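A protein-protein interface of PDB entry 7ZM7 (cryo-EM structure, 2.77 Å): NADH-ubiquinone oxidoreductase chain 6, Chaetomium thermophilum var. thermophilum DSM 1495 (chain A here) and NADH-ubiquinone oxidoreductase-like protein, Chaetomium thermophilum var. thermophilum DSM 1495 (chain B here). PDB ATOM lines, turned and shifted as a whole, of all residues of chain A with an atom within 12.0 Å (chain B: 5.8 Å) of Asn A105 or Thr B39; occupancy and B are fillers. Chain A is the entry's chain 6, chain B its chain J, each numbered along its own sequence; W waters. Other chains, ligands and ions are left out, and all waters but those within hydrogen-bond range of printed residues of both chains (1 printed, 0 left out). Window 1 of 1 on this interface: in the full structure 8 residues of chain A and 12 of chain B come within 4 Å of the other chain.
Of the 16 printed residues of chain A, 7 touch a printed residue of chain B.
Hydrophobic or aromatic side chains of chain B within 4 Å of the printed part of chain A: Ala B36, Val B46, Pro B48 and Ile B51.
Among the printed residues, 15 pairs touch across the chains.
Among the printed residues, no Asp or Glu carboxylate lies within 4 Å of a Lys or Arg side-chain nitrogen of the other chain.
Among the printed residues, merely in contact across the chains: Ser A104 with Asn B45, Ser A104 with Pro B48, Asn A105 with Thr B39, Asn A105 with Val B46, Pro A108 with Pro B48, Pro A108 with Ile B51, Leu A109 with Ala B36, Leu A109 with Val B37, Leu A109 with Ser B40 and Leu A112 with Ala B36.
OG of Ser B40 is in hydrogen-bond range of OG of Ser A106, 3.0 Å away.
The backbone carbonyl oxygen (O) of Lys B44 sits close to the side-chain amide nitrogen (ND2) of Asn A102.
ND2 of Asn A105 lies within hydrogen-bond range of O of Lys B44 (3.1 Å).
The side-chain amide oxygen (OD1) of Asn A102 is in hydrogen-bond range of the side-chain amide nitrogen (ND2) of Asn B45 (2.8 Å).
The backbone NH (N) of Gly B47 is in hydrogen-bond range of the side-chain amide oxygen (OD1) of Asn A105 (2.7 Å).
The backbone carbonyl oxygen (O) of Ala B35 lies close to the side-chain hydroxyl (OG1) of Thr B39, at 3.4 Å.
O of Ala B36 lies within hydrogen-bond range of OG1 of Thr B39, 3.0 Å away.
OG1 of Thr A110 is in hydrogen-bond range of O of Ser A106 (2.7 Å).
Of the printed residues of chain B, Asn A105 touches Thr B39 (3.3 Å), Lys B44 (3.1 Å), Val B46 (3.5 Å) and Gly B47 (2.7 Å).
Of chain A, only Asn A105 (3.3 Å) comes within 4 Å of Thr B39.
No residue of chain A comes within 4 Å of Ala B35.
Of the printed residues of chain A, Val B37 touches Leu A109.
No residue of chain A comes within 4 Å of Arg B38.
No residue of chain A comes within 4 Å of Leu B41.
Asn B45 touches just these residues of chain A: Asn A102 (2.8 Å) and Ser A104 (3.8 Å).
Val B46 touches just one residue of chain A: Asn A105 (3.5 Å).
Of chain A, only Ser A104 and Pro A108 come within 4 Å of Pro B48.
No residue of chain A comes within 4 Å of Ala B50.
Ile B51 touches one residue of chain A.
Arg B54 touches none of the printed residues of chain A.
Printed residues of chain B within 4 Å of Leu A109: Ala B36, Val B37 and Ser B40.
Of the printed residues of chain B, Asn A102 touches Lys B44 and Asn B45.
Printed residues of chain B within 4 Å of Ser A104: Asn B45 (3.8 Å) and Pro B48 (3.3 Å).
Of the printed residues of chain A, Lys B44 touches Asn A102 and Asn A105.
Ser A101 touches none of the printed residues of chain B.
The nearest residue of chain B that does not touch Asn A105 is Ala B42 (4.2 Å).
Water W1 lies within hydrogen-bond range of O of Asn A105 (2.8 Å), N of Leu A109 (2.9 Å), OG1 of Thr B39 (2.9 Å) and O of Ala B36 (3.1 Å).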
ATOM      1  N   ILE A  38      31.882   3.808  13.928  1.00  0.00           N
ATOM      2  CA  ILE A  38      30.636   4.266  14.526  1.00  0.00           C
ATOM      3  C   ILE A  38      30.233   5.659  14.077  1.00  0.00           C
ATOM      4  O   ILE A  38      29.259   6.209  14.605  1.00  0.00           O
ATOM      5  CB  ILE A  38      30.708   4.226  16.068  1.00  0.00           C
ATOM      6  CG1 ILE A  38      31.737   5.220  16.584  1.00  0.00           C
ATOM      7  CG2 ILE A  38      31.007   2.835  16.559  1.00  0.00           C
ATOM      8  CD1 ILE A  38      31.590   5.541  18.015  1.00  0.00           C
ATOM      9  N   ILE A  39      30.945   6.252  13.126  1.00  0.00           N
ATOM     10  CA  ILE A  39      30.559   7.544  12.565  1.00  0.00           C
ATOM     11  C   ILE A  39      30.258   7.473  11.080  1.00  0.00           C
ATOM     12  O   ILE A  39      29.585   8.375  10.560  1.00  0.00           O
ATOM     13  CB  ILE A  39      31.631   8.619  12.831  1.00  0.00           C
ATOM     14  CG1 ILE A  39      32.891   8.296  12.032  1.00  0.00           C
ATOM     15  CG2 ILE A  39      31.903   8.725  14.290  1.00  0.00           C
ATOM     16  CD1 ILE A  39      33.925   9.367  12.021  1.00  0.00           C
ATOM     17  N   GLN A 100      20.612   7.398   8.811  1.00  0.00           N
ATOM     18  CA  GLN A 100      21.337   8.545   9.321  1.00  0.00           C
ATOM     19  C   GLN A 100      20.476   9.248  10.356  1.00  0.00           C
ATOM     20  O   GLN A 100      19.353   9.668  10.059  1.00  0.00           O
ATOM     21  CB  GLN A 100      21.717   9.499   8.189  1.00  0.00           C
ATOM     22  CG  GLN A 100      22.532  10.680   8.656  1.00  0.00           C
ATOM     23  CD  GLN A 100      23.722  10.251   9.485  1.00  0.00           C
ATOM     24  OE1 GLN A 100      24.390   9.267   9.172  1.00  0.00           O
ATOM     25  NE2 GLN A 100      23.986  10.983  10.559  1.00  0.00           N
ATOM     26  N   SER A 101      21.006   9.379  11.561  1.00  0.00           N
ATOM     27  CA  SER A 101      20.330  10.061  12.648  1.00  0.00           C
ATOM     28  C   SER A 101      21.109  11.315  13.011  1.00  0.00           C
ATOM     29  O   SER A 101      22.288  11.461  12.681  1.00  0.00           O
ATOM     30  CB  SER A 101      20.187   9.144  13.861  1.00  0.00           C
ATOM     31  OG  SER A 101      21.446   8.839  14.416  1.00  0.00           O
ATOM     32  N   ASN A 102      20.432  12.222  13.705  1.00  0.00           N
ATOM     33  CA  ASN A 102      21.055  13.473  14.122  1.00  0.00           C
ATOM     34  C   ASN A 102      22.091  13.155  15.184  1.00  0.00           C
ATOM     35  O   ASN A 102      21.773  13.039  16.367  1.00  0.00           O
ATOM     36  CB  ASN A 102      20.003  14.440  14.648  1.00  0.00           C
ATOM     37  CG  ASN A 102      19.107  14.968  13.556  1.00  0.00           C
ATOM     38  OD1 ASN A 102      19.582  15.448  12.529  1.00  0.00           O
ATOM     39  ND2 ASN A 102      17.799  14.884  13.767  1.00  0.00           N
ATOM     40  N   THR A 103      23.345  13.022  14.758  1.00  0.00           N
ATOM     41  CA  THR A 103      24.409  12.629  15.670  1.00  0.00           C
ATOM     42  C   THR A 103      24.822  13.765  16.590  1.00  0.00           C
ATOM     43  O   THR A 103      25.376  13.514  17.665  1.00  0.00           O
ATOM     44  CB  THR A 103      25.623  12.155  14.880  1.00  0.00           C
ATOM     45  OG1 THR A 103      25.933  13.128  13.878  1.00  0.00           O
ATOM     46  CG2 THR A 103      25.333  10.822  14.213  1.00  0.00           C
ATOM     47  N   SER A 104      24.572  15.009  16.181  1.00  0.00           N
ATOM     48  CA  SER A 104      25.046  16.153  16.947  1.00  0.00           C
ATOM     49  C   SER A 104      24.344  16.262  18.288  1.00  0.00           C
ATOM     50  O   SER A 104      24.875  16.875  19.219  1.00  0.00           O
ATOM     51  CB  SER A 104      24.851  17.426  16.136  1.00  0.00           C
ATOM     52  OG  SER A 104      23.527  17.502  15.638  1.00  0.00           O
ATOM     53  N   ASN A 105      23.155  15.680  18.407  1.00  0.00           N
ATOM     54  CA  ASN A 105      22.420  15.741  19.661  1.00  0.00           C
ATOM     55  C   ASN A 105      23.122  14.946  20.743  1.00  0.00           C
ATOM     56  O   ASN A 105      23.120  15.336  21.913  1.00  0.00           O
ATOM     57  CB  ASN A 105      21.011  15.206  19.457  1.00  0.00           C
ATOM     58  CG  ASN A 105      20.245  16.015  18.489  1.00  0.00           C
ATOM     59  OD1 ASN A 105      20.549  17.177  18.279  1.00  0.00           O
ATOM     60  ND2 ASN A 105      19.256  15.411  17.864  1.00  0.00           N
ATOM     61  N   SER A 106      23.735  13.836  20.363  1.00  0.00           N
ATOM     62  CA  SER A 106      24.238  12.852  21.292  1.00  0.00           C
ATOM     63  C   SER A 106      25.669  13.134  21.709  1.00  0.00           C
ATOM     64  O   SER A 106      26.286  12.305  22.385  1.00  0.00           O
ATOM     65  CB  SER A 106      24.120  11.481  20.660  1.00  0.00           C
ATOM     66  OG  SER A 106      22.804  11.271  20.216  1.00  0.00           O
ATOM     67  N   ILE A 107      26.212  14.275  21.299  1.00  0.00           N
ATOM     68  CA  ILE A 107      27.526  14.685  21.785  1.00  0.00           C
ATOM     69  C   ILE A 107      27.547  14.865  23.299  1.00  0.00           C
ATOM     70  O   ILE A 107      28.477  14.356  23.943  1.00  0.00           O
ATOM     71  CB  ILE A 107      27.994  15.941  21.028  1.00  0.00           C
ATOM     72  CG1 ILE A 107      28.399  15.579  19.602  1.00  0.00           C
ATOM     73  CG2 ILE A 107      29.134  16.623  21.765  1.00  0.00           C
ATOM     74  CD1 ILE A 107      29.570  14.628  19.529  1.00  0.00           C
ATOM     75  N   PRO A 108      26.600  15.577  23.924  1.00  0.00           N
ATOM     76  CA  PRO A 108      26.636  15.680  25.389  1.00  0.00           C
ATOM     77  C   PRO A 108      26.562  14.346  26.094  1.00  0.00           C
ATOM     78  O   PRO A 108      27.256  14.145  27.098  1.00  0.00           O
ATOM     79  CB  PRO A 108      25.416  16.550  25.702  1.00  0.00           C
ATOM     80  CG  PRO A 108      25.203  17.332  24.482  1.00  0.00           C
ATOM     81  CD  PRO A 108      25.539  16.425  23.361  1.00  0.00           C
ATOM     82  N   LEU A 109      25.739  13.420  25.598  1.00  0.00           N
ATOM     83  CA  LEU A 109      25.660  12.110  26.220  1.00  0.00           C
ATOM     84  C   LEU A 109      26.901  11.288  25.922  1.00  0.00           C
ATOM     85  O   LEU A 109      27.255  10.401  26.705  1.00  0.00           O
ATOM     86  CB  LEU A 109      24.408  11.378  25.748  1.00  0.00           C
ATOM     87  CG  LEU A 109      23.948  10.129  26.503  1.00  0.00           C
ATOM     88  CD1 LEU A 109      24.008  10.339  27.995  1.00  0.00           C
ATOM     89  CD2 LEU A 109      22.550   9.752  26.070  1.00  0.00           C
ATOM     90  N   THR A 110      27.551  11.537  24.785  1.00  0.00           N
ATOM     91  CA  THR A 110      28.866  10.956  24.546  1.00  0.00           C
ATOM     92  C   THR A 110      29.883  11.498  25.537  1.00  0.00           C
ATOM     93  O   THR A 110      30.722  10.752  26.050  1.00  0.00           O
ATOM     94  CB  THR A 110      29.310  11.217  23.106  1.00  0.00           C
ATOM     95  OG1 THR A 110      28.378  10.622  22.201  1.00  0.00           O
ATOM     96  CG2 THR A 110      30.702  10.660  22.841  1.00  0.00           C
ATOM     97  N   ILE A 111      29.816  12.793  25.829  1.00  0.00           N
ATOM     98  CA  ILE A 111      30.732  13.384  26.799  1.00  0.00           C
ATOM     99  C   ILE A 111      30.516  12.775  28.175  1.00  0.00           C
ATOM    100  O   ILE A 111      31.472  12.419  28.873  1.00  0.00           O
ATOM    101  CB  ILE A 111      30.557  14.914  26.826  1.00  0.00           C
ATOM    102  CG1 ILE A 111      30.992  15.524  25.496  1.00  0.00           C
ATOM    103  CG2 ILE A 111      31.355  15.518  27.960  1.00  0.00           C
ATOM    104  CD1 ILE A 111      30.529  16.949  25.303  1.00  0.00           C
ATOM    105  N   LEU A 112      29.255  12.633  28.581  1.00  0.00           N
ATOM    106  CA  LEU A 112      28.951  12.180  29.932  1.00  0.00           C
ATOM    107  C   LEU A 112      29.336  10.721  30.131  1.00  0.00           C
ATOM    108  O   LEU A 112      30.010  10.374  31.107  1.00  0.00           O
ATOM    109  CB  LEU A 112      27.470  12.393  30.222  1.00  0.00           C
ATOM    110  CG  LEU A 112      27.099  13.860  30.441  1.00  0.00           C
ATOM    111  CD1 LEU A 112      25.655  13.999  30.889  1.00  0.00           C
ATOM    112  CD2 LEU A 112      28.039  14.505  31.446  1.00  0.00           C
ATOM    113  N   VAL A 113      28.927   9.850  29.211  1.00  0.00           N
ATOM    114  CA  VAL A 113      29.148   8.423  29.412  1.00  0.00           C
ATOM    115  C   VAL A 113      30.618   8.066  29.199  1.00  0.00           C
ATOM    116  O   VAL A 113      31.116   7.078  29.745  1.00  0.00           O
ATOM    117  CB  VAL A 113      28.209   7.609  28.506  1.00  0.00           C
ATOM    118  CG1 VAL A 113      28.398   6.117  28.736  1.00  0.00           C
ATOM    119  CG2 VAL A 113      26.778   8.010  28.774  1.00  0.00           C
ATOM    120  N   PHE B  34      20.235  12.894  32.752  1.00  0.00           N
ATOM    121  CA  PHE B  34      18.899  12.605  32.245  1.00  0.00           C
ATOM    122  C   PHE B  34      18.547  13.514  31.079  1.00  0.00           C
ATOM    123  O   PHE B  34      17.989  13.059  30.077  1.00  0.00           O
ATOM    124  CB  PHE B  34      17.880  12.731  33.364  1.00  0.00           C
ATOM    125  CG  PHE B  34      17.666  11.459  34.112  1.00  0.00           C
ATOM    126  CD1 PHE B  34      17.257  10.318  33.449  1.00  0.00           C
ATOM    127  CD2 PHE B  34      17.907  11.390  35.469  1.00  0.00           C
ATOM    128  CE1 PHE B  34      17.069   9.139  34.131  1.00  0.00           C
ATOM    129  CE2 PHE B  34      17.722  10.216  36.156  1.00  0.00           C
ATOM    130  CZ  PHE B  34      17.302   9.087  35.487  1.00  0.00           C
ATOM    131  N   ALA B  35      18.895  14.793  31.179  1.00  0.00           N
ATOM    132  CA  ALA B  35      18.697  15.703  30.063  1.00  0.00           C
ATOM    133  C   ALA B  35      19.530  15.289  28.860  1.00  0.00           C
ATOM    134  O   ALA B  35      19.150  15.550  27.713  1.00  0.00           O
ATOM    135  CB  ALA B  35      19.042  17.125  30.492  1.00  0.00           C
ATOM    136  N   ALA B  36      20.682  14.660  29.098  1.00  0.00           N
ATOM    137  CA  ALA B  36      21.475  14.147  27.991  1.00  0.00           C
ATOM    138  C   ALA B  36      20.733  13.038  27.254  1.00  0.00           C
ATOM    139  O   ALA B  36      20.830  12.917  26.030  1.00  0.00           O
ATOM    140  CB  ALA B  36      22.820  13.653  28.501  1.00  0.00           C
ATOM    141  N   VAL B  37      19.995  12.214  27.992  1.00  0.00           N
ATOM    142  CA  VAL B  37      19.172  11.180  27.380  1.00  0.00           C
ATOM    143  C   VAL B  37      18.056  11.811  26.568  1.00  0.00           C
ATOM    144  O   VAL B  37      17.705  11.330  25.486  1.00  0.00           O
ATOM    145  CB  VAL B  37      18.620  10.250  28.473  1.00  0.00           C
ATOM    146  CG1 VAL B  37      17.713   9.200  27.877  1.00  0.00           C
ATOM    147  CG2 VAL B  37      19.761   9.620  29.241  1.00  0.00           C
ATOM    148  N   ARG B  38      17.470  12.891  27.091  1.00  0.00           N
ATOM    149  CA  ARG B  38      16.364  13.560  26.418  1.00  0.00           C
ATOM    150  C   ARG B  38      16.788  14.130  25.077  1.00  0.00           C
ATOM    151  O   ARG B  38      16.040  14.054  24.100  1.00  0.00           O
ATOM    152  CB  ARG B  38      15.806  14.661  27.311  1.00  0.00           C
ATOM    153  CG  ARG B  38      15.185  14.206  28.618  1.00  0.00           C
ATOM    154  CD  ARG B  38      13.917  13.432  28.343  1.00  0.00           C
ATOM    155  NE  ARG B  38      12.950  14.266  27.639  1.00  0.00           N
ATOM    156  CZ  ARG B  38      12.088  15.083  28.232  1.00  0.00           C
ATOM    157  NH1 ARG B  38      12.062  15.178  29.554  1.00  0.00           N
ATOM    158  NH2 ARG B  38      11.252  15.804  27.502  1.00  0.00           N
ATOM    159  N   THR B  39      17.975  14.721  25.019  1.00  0.00           N
ATOM    160  CA  THR B  39      18.449  15.308  23.777  1.00  0.00           C
ATOM    161  C   THR B  39      18.875  14.238  22.791  1.00  0.00           C
ATOM    162  O   THR B  39      18.621  14.358  21.588  1.00  0.00           O
ATOM    163  CB  THR B  39      19.602  16.264  24.059  1.00  0.00           C
ATOM    164  OG1 THR B  39      20.678  15.541  24.652  1.00  0.00           O
ATOM    165  CG2 THR B  39      19.169  17.340  25.005  1.00  0.00           C
ATOM    166  N   SER B  40      19.528  13.187  23.281  1.00  0.00           N
ATOM    167  CA  SER B  40      19.929  12.104  22.396  1.00  0.00           C
ATOM    168  C   SER B  40      18.720  11.448  21.752  1.00  0.00           C
ATOM    169  O   SER B  40      18.784  11.038  20.590  1.00  0.00           O
ATOM    170  CB  SER B  40      20.756  11.083  23.163  1.00  0.00           C
ATOM    171  OG  SER B  40      21.129  10.014  22.328  1.00  0.00           O
ATOM    172  N   LEU B  41      17.609  11.359  22.477  1.00  0.00           N
ATOM    173  CA  LEU B  41      16.386  10.779  21.944  1.00  0.00           C
ATOM    174  C   LEU B  41      15.457  11.798  21.315  1.00  0.00           C
ATOM    175  O   LEU B  41      14.356  11.428  20.902  1.00  0.00           O
ATOM    176  CB  LEU B  41      15.628  10.005  23.020  1.00  0.00           C
ATOM    177  CG  LEU B  41      16.294   8.721  23.498  1.00  0.00           C
ATOM    178  CD1 LEU B  41      15.501   8.079  24.617  1.00  0.00           C
ATOM    179  CD2 LEU B  41      16.473   7.778  22.333  1.00  0.00           C
ATOM    180  N   ALA B  42      15.866  13.055  21.223  1.00  0.00           N
ATOM    181  CA  ALA B  42      15.086  14.031  20.479  1.00  0.00           C
ATOM    182  C   ALA B  42      14.916  13.571  19.039  1.00  0.00           C
ATOM    183  O   ALA B  42      15.847  13.048  18.425  1.00  0.00           O
ATOM    184  CB  ALA B  42      15.768  15.395  20.521  1.00  0.00           C
ATOM    185  N   LYS B  44      14.098  15.509  16.451  1.00  0.00           N
ATOM    186  CA  LYS B  44      14.456  16.539  15.492  1.00  0.00           C
ATOM    187  C   LYS B  44      15.927  16.900  15.642  1.00  0.00           C
ATOM    188  O   LYS B  44      16.636  16.392  16.514  1.00  0.00           O
ATOM    189  CB  LYS B  44      13.583  17.784  15.664  1.00  0.00           C
ATOM    190  CG  LYS B  44      12.134  17.575  15.277  1.00  0.00           C
ATOM    191  CD  LYS B  44      11.314  18.822  15.538  1.00  0.00           C
ATOM    192  CE  LYS B  44      11.680  19.920  14.556  1.00  0.00           C
ATOM    193  NZ  LYS B  44      11.269  19.584  13.167  1.00  0.00           N
ATOM    194  N   ASN B  45      16.383  17.788  14.761  1.00  0.00           N
ATOM    195  CA  ASN B  45      17.760  18.275  14.792  1.00  0.00           C
ATOM    196  C   ASN B  45      17.826  19.439  15.773  1.00  0.00           C
ATOM    197  O   ASN B  45      17.891  20.612  15.403  1.00  0.00           O
ATOM    198  CB  ASN B  45      18.216  18.681  13.396  1.00  0.00           C
ATOM    199  CG  ASN B  45      19.721  18.678  13.251  1.00  0.00           C
ATOM    200  OD1 ASN B  45      20.440  19.154  14.127  1.00  0.00           O
ATOM    201  ND2 ASN B  45      20.207  18.137  12.141  1.00  0.00           N
ATOM    202  N   VAL B  46      17.812  19.096  17.064  1.00  0.00           N
ATOM    203  CA  VAL B  46      17.756  20.113  18.112  1.00  0.00           C
ATOM    204  C   VAL B  46      19.124  20.622  18.537  1.00  0.00           C
ATOM    205  O   VAL B  46      19.207  21.695  19.151  1.00  0.00           O
ATOM    206  CB  VAL B  46      17.004  19.583  19.346  1.00  0.00           C
ATOM    207  CG1 VAL B  46      15.655  19.019  18.935  1.00  0.00           C
ATOM    208  CG2 VAL B  46      17.838  18.537  20.054  1.00  0.00           C
ATOM    209  N   GLY B  47      20.194  19.894  18.241  1.00  0.00           N
ATOM    210  CA  GLY B  47      21.529  20.366  18.508  1.00  0.00           C
ATOM    211  C   GLY B  47      22.046  19.991  19.880  1.00  0.00           C
ATOM    212  O   GLY B  47      21.305  19.521  20.748  1.00  0.00           O
ATOM    213  N   PRO B  48      23.346  20.203  20.101  1.00  0.00           N
ATOM    214  CA  PRO B  48      23.938  19.817  21.387  1.00  0.00           C
ATOM    215  C   PRO B  48      23.569  20.754  22.518  1.00  0.00           C
ATOM    216  O   PRO B  48      23.351  20.292  23.644  1.00  0.00           O
ATOM    217  CB  PRO B  48      25.450  19.859  21.110  1.00  0.00           C
ATOM    218  CG  PRO B  48      25.591  20.110  19.624  1.00  0.00           C
ATOM    219  CD  PRO B  48      24.340  20.789  19.194  1.00  0.00           C
ATOM    220  N   ALA B  50      20.919  22.193  23.134  1.00  0.00           N
ATOM    221  CA  ALA B  50      19.553  22.026  23.603  1.00  0.00           C
ATOM    222  C   ALA B  50      19.496  21.393  24.983  1.00  0.00           C
ATOM    223  O   ALA B  50      18.461  21.488  25.653  1.00  0.00           O
ATOM    224  CB  ALA B  50      18.758  21.179  22.610  1.00  0.00           C
ATOM    225  N   ILE B  51      20.578  20.744  25.419  1.00  0.00           N
ATOM    226  CA  ILE B  51      20.602  20.148  26.748  1.00  0.00           C
ATOM    227  C   ILE B  51      20.503  21.221  27.819  1.00  0.00           C
ATOM    228  O   ILE B  51      20.015  20.963  28.925  1.00  0.00           O
ATOM    229  CB  ILE B  51      21.866  19.284  26.923  1.00  0.00           C
ATOM    230  CG1 ILE B  51      21.752  18.411  28.171  1.00  0.00           C
ATOM    231  CG2 ILE B  51      23.109  20.149  26.998  1.00  0.00           C
ATOM    232  CD1 ILE B  51      22.859  17.411  28.295  1.00  0.00           C
ATOM    233  N   ARG B  54      16.454  23.381  26.054  1.00  0.00           N
ATOM    234  CA  ARG B  54      15.173  22.686  26.021  1.00  0.00           C
ATOM    235  C   ARG B  54      14.971  21.810  27.253  1.00  0.00           C
ATOM    236  O   ARG B  54      13.850  21.702  27.760  1.00  0.00           O
ATOM    237  CB  ARG B  54      15.070  21.853  24.744  1.00  0.00           C
ATOM    238  CG  ARG B  54      15.089  22.688  23.471  1.00  0.00           C
ATOM    239  CD  ARG B  54      14.964  21.833  22.219  1.00  0.00           C
ATOM    240  NE  ARG B  54      13.665  21.175  22.116  1.00  0.00           N
ATOM    241  CZ  ARG B  54      13.496  19.858  22.077  1.00  0.00           C
ATOM    242  NH1 ARG B  54      14.546  19.048  22.129  1.00  0.00           N
ATOM    243  NH2 ARG B  54      12.276  19.349  21.981  1.00  0.00           N
ATOM    244  N   ASN B  55      16.036  21.179  27.751  1.00  0.00           N
ATOM    245  CA  ASN B  55      15.941  20.294  28.905  1.00  0.00           C
ATOM    246  C   ASN B  55      16.635  20.864  30.135  1.00  0.00           C
ATOM    247  O   ASN B  55      16.862  20.133  31.102  1.00  0.00           O
ATOM    248  CB  ASN B  55      16.520  18.917  28.582  1.00  0.00           C
ATOM    249  CG  ASN B  55      15.866  18.277  27.381  1.00  0.00           C
ATOM    250  OD1 ASN B  55      16.513  17.568  26.618  1.00  0.00           O
ATOM    251  ND2 ASN B  55      14.573  18.523  27.207  1.00  0.00           N
HETATM  252  O   HOH W   1      23.184  14.069  24.438  1.00  0.00           O
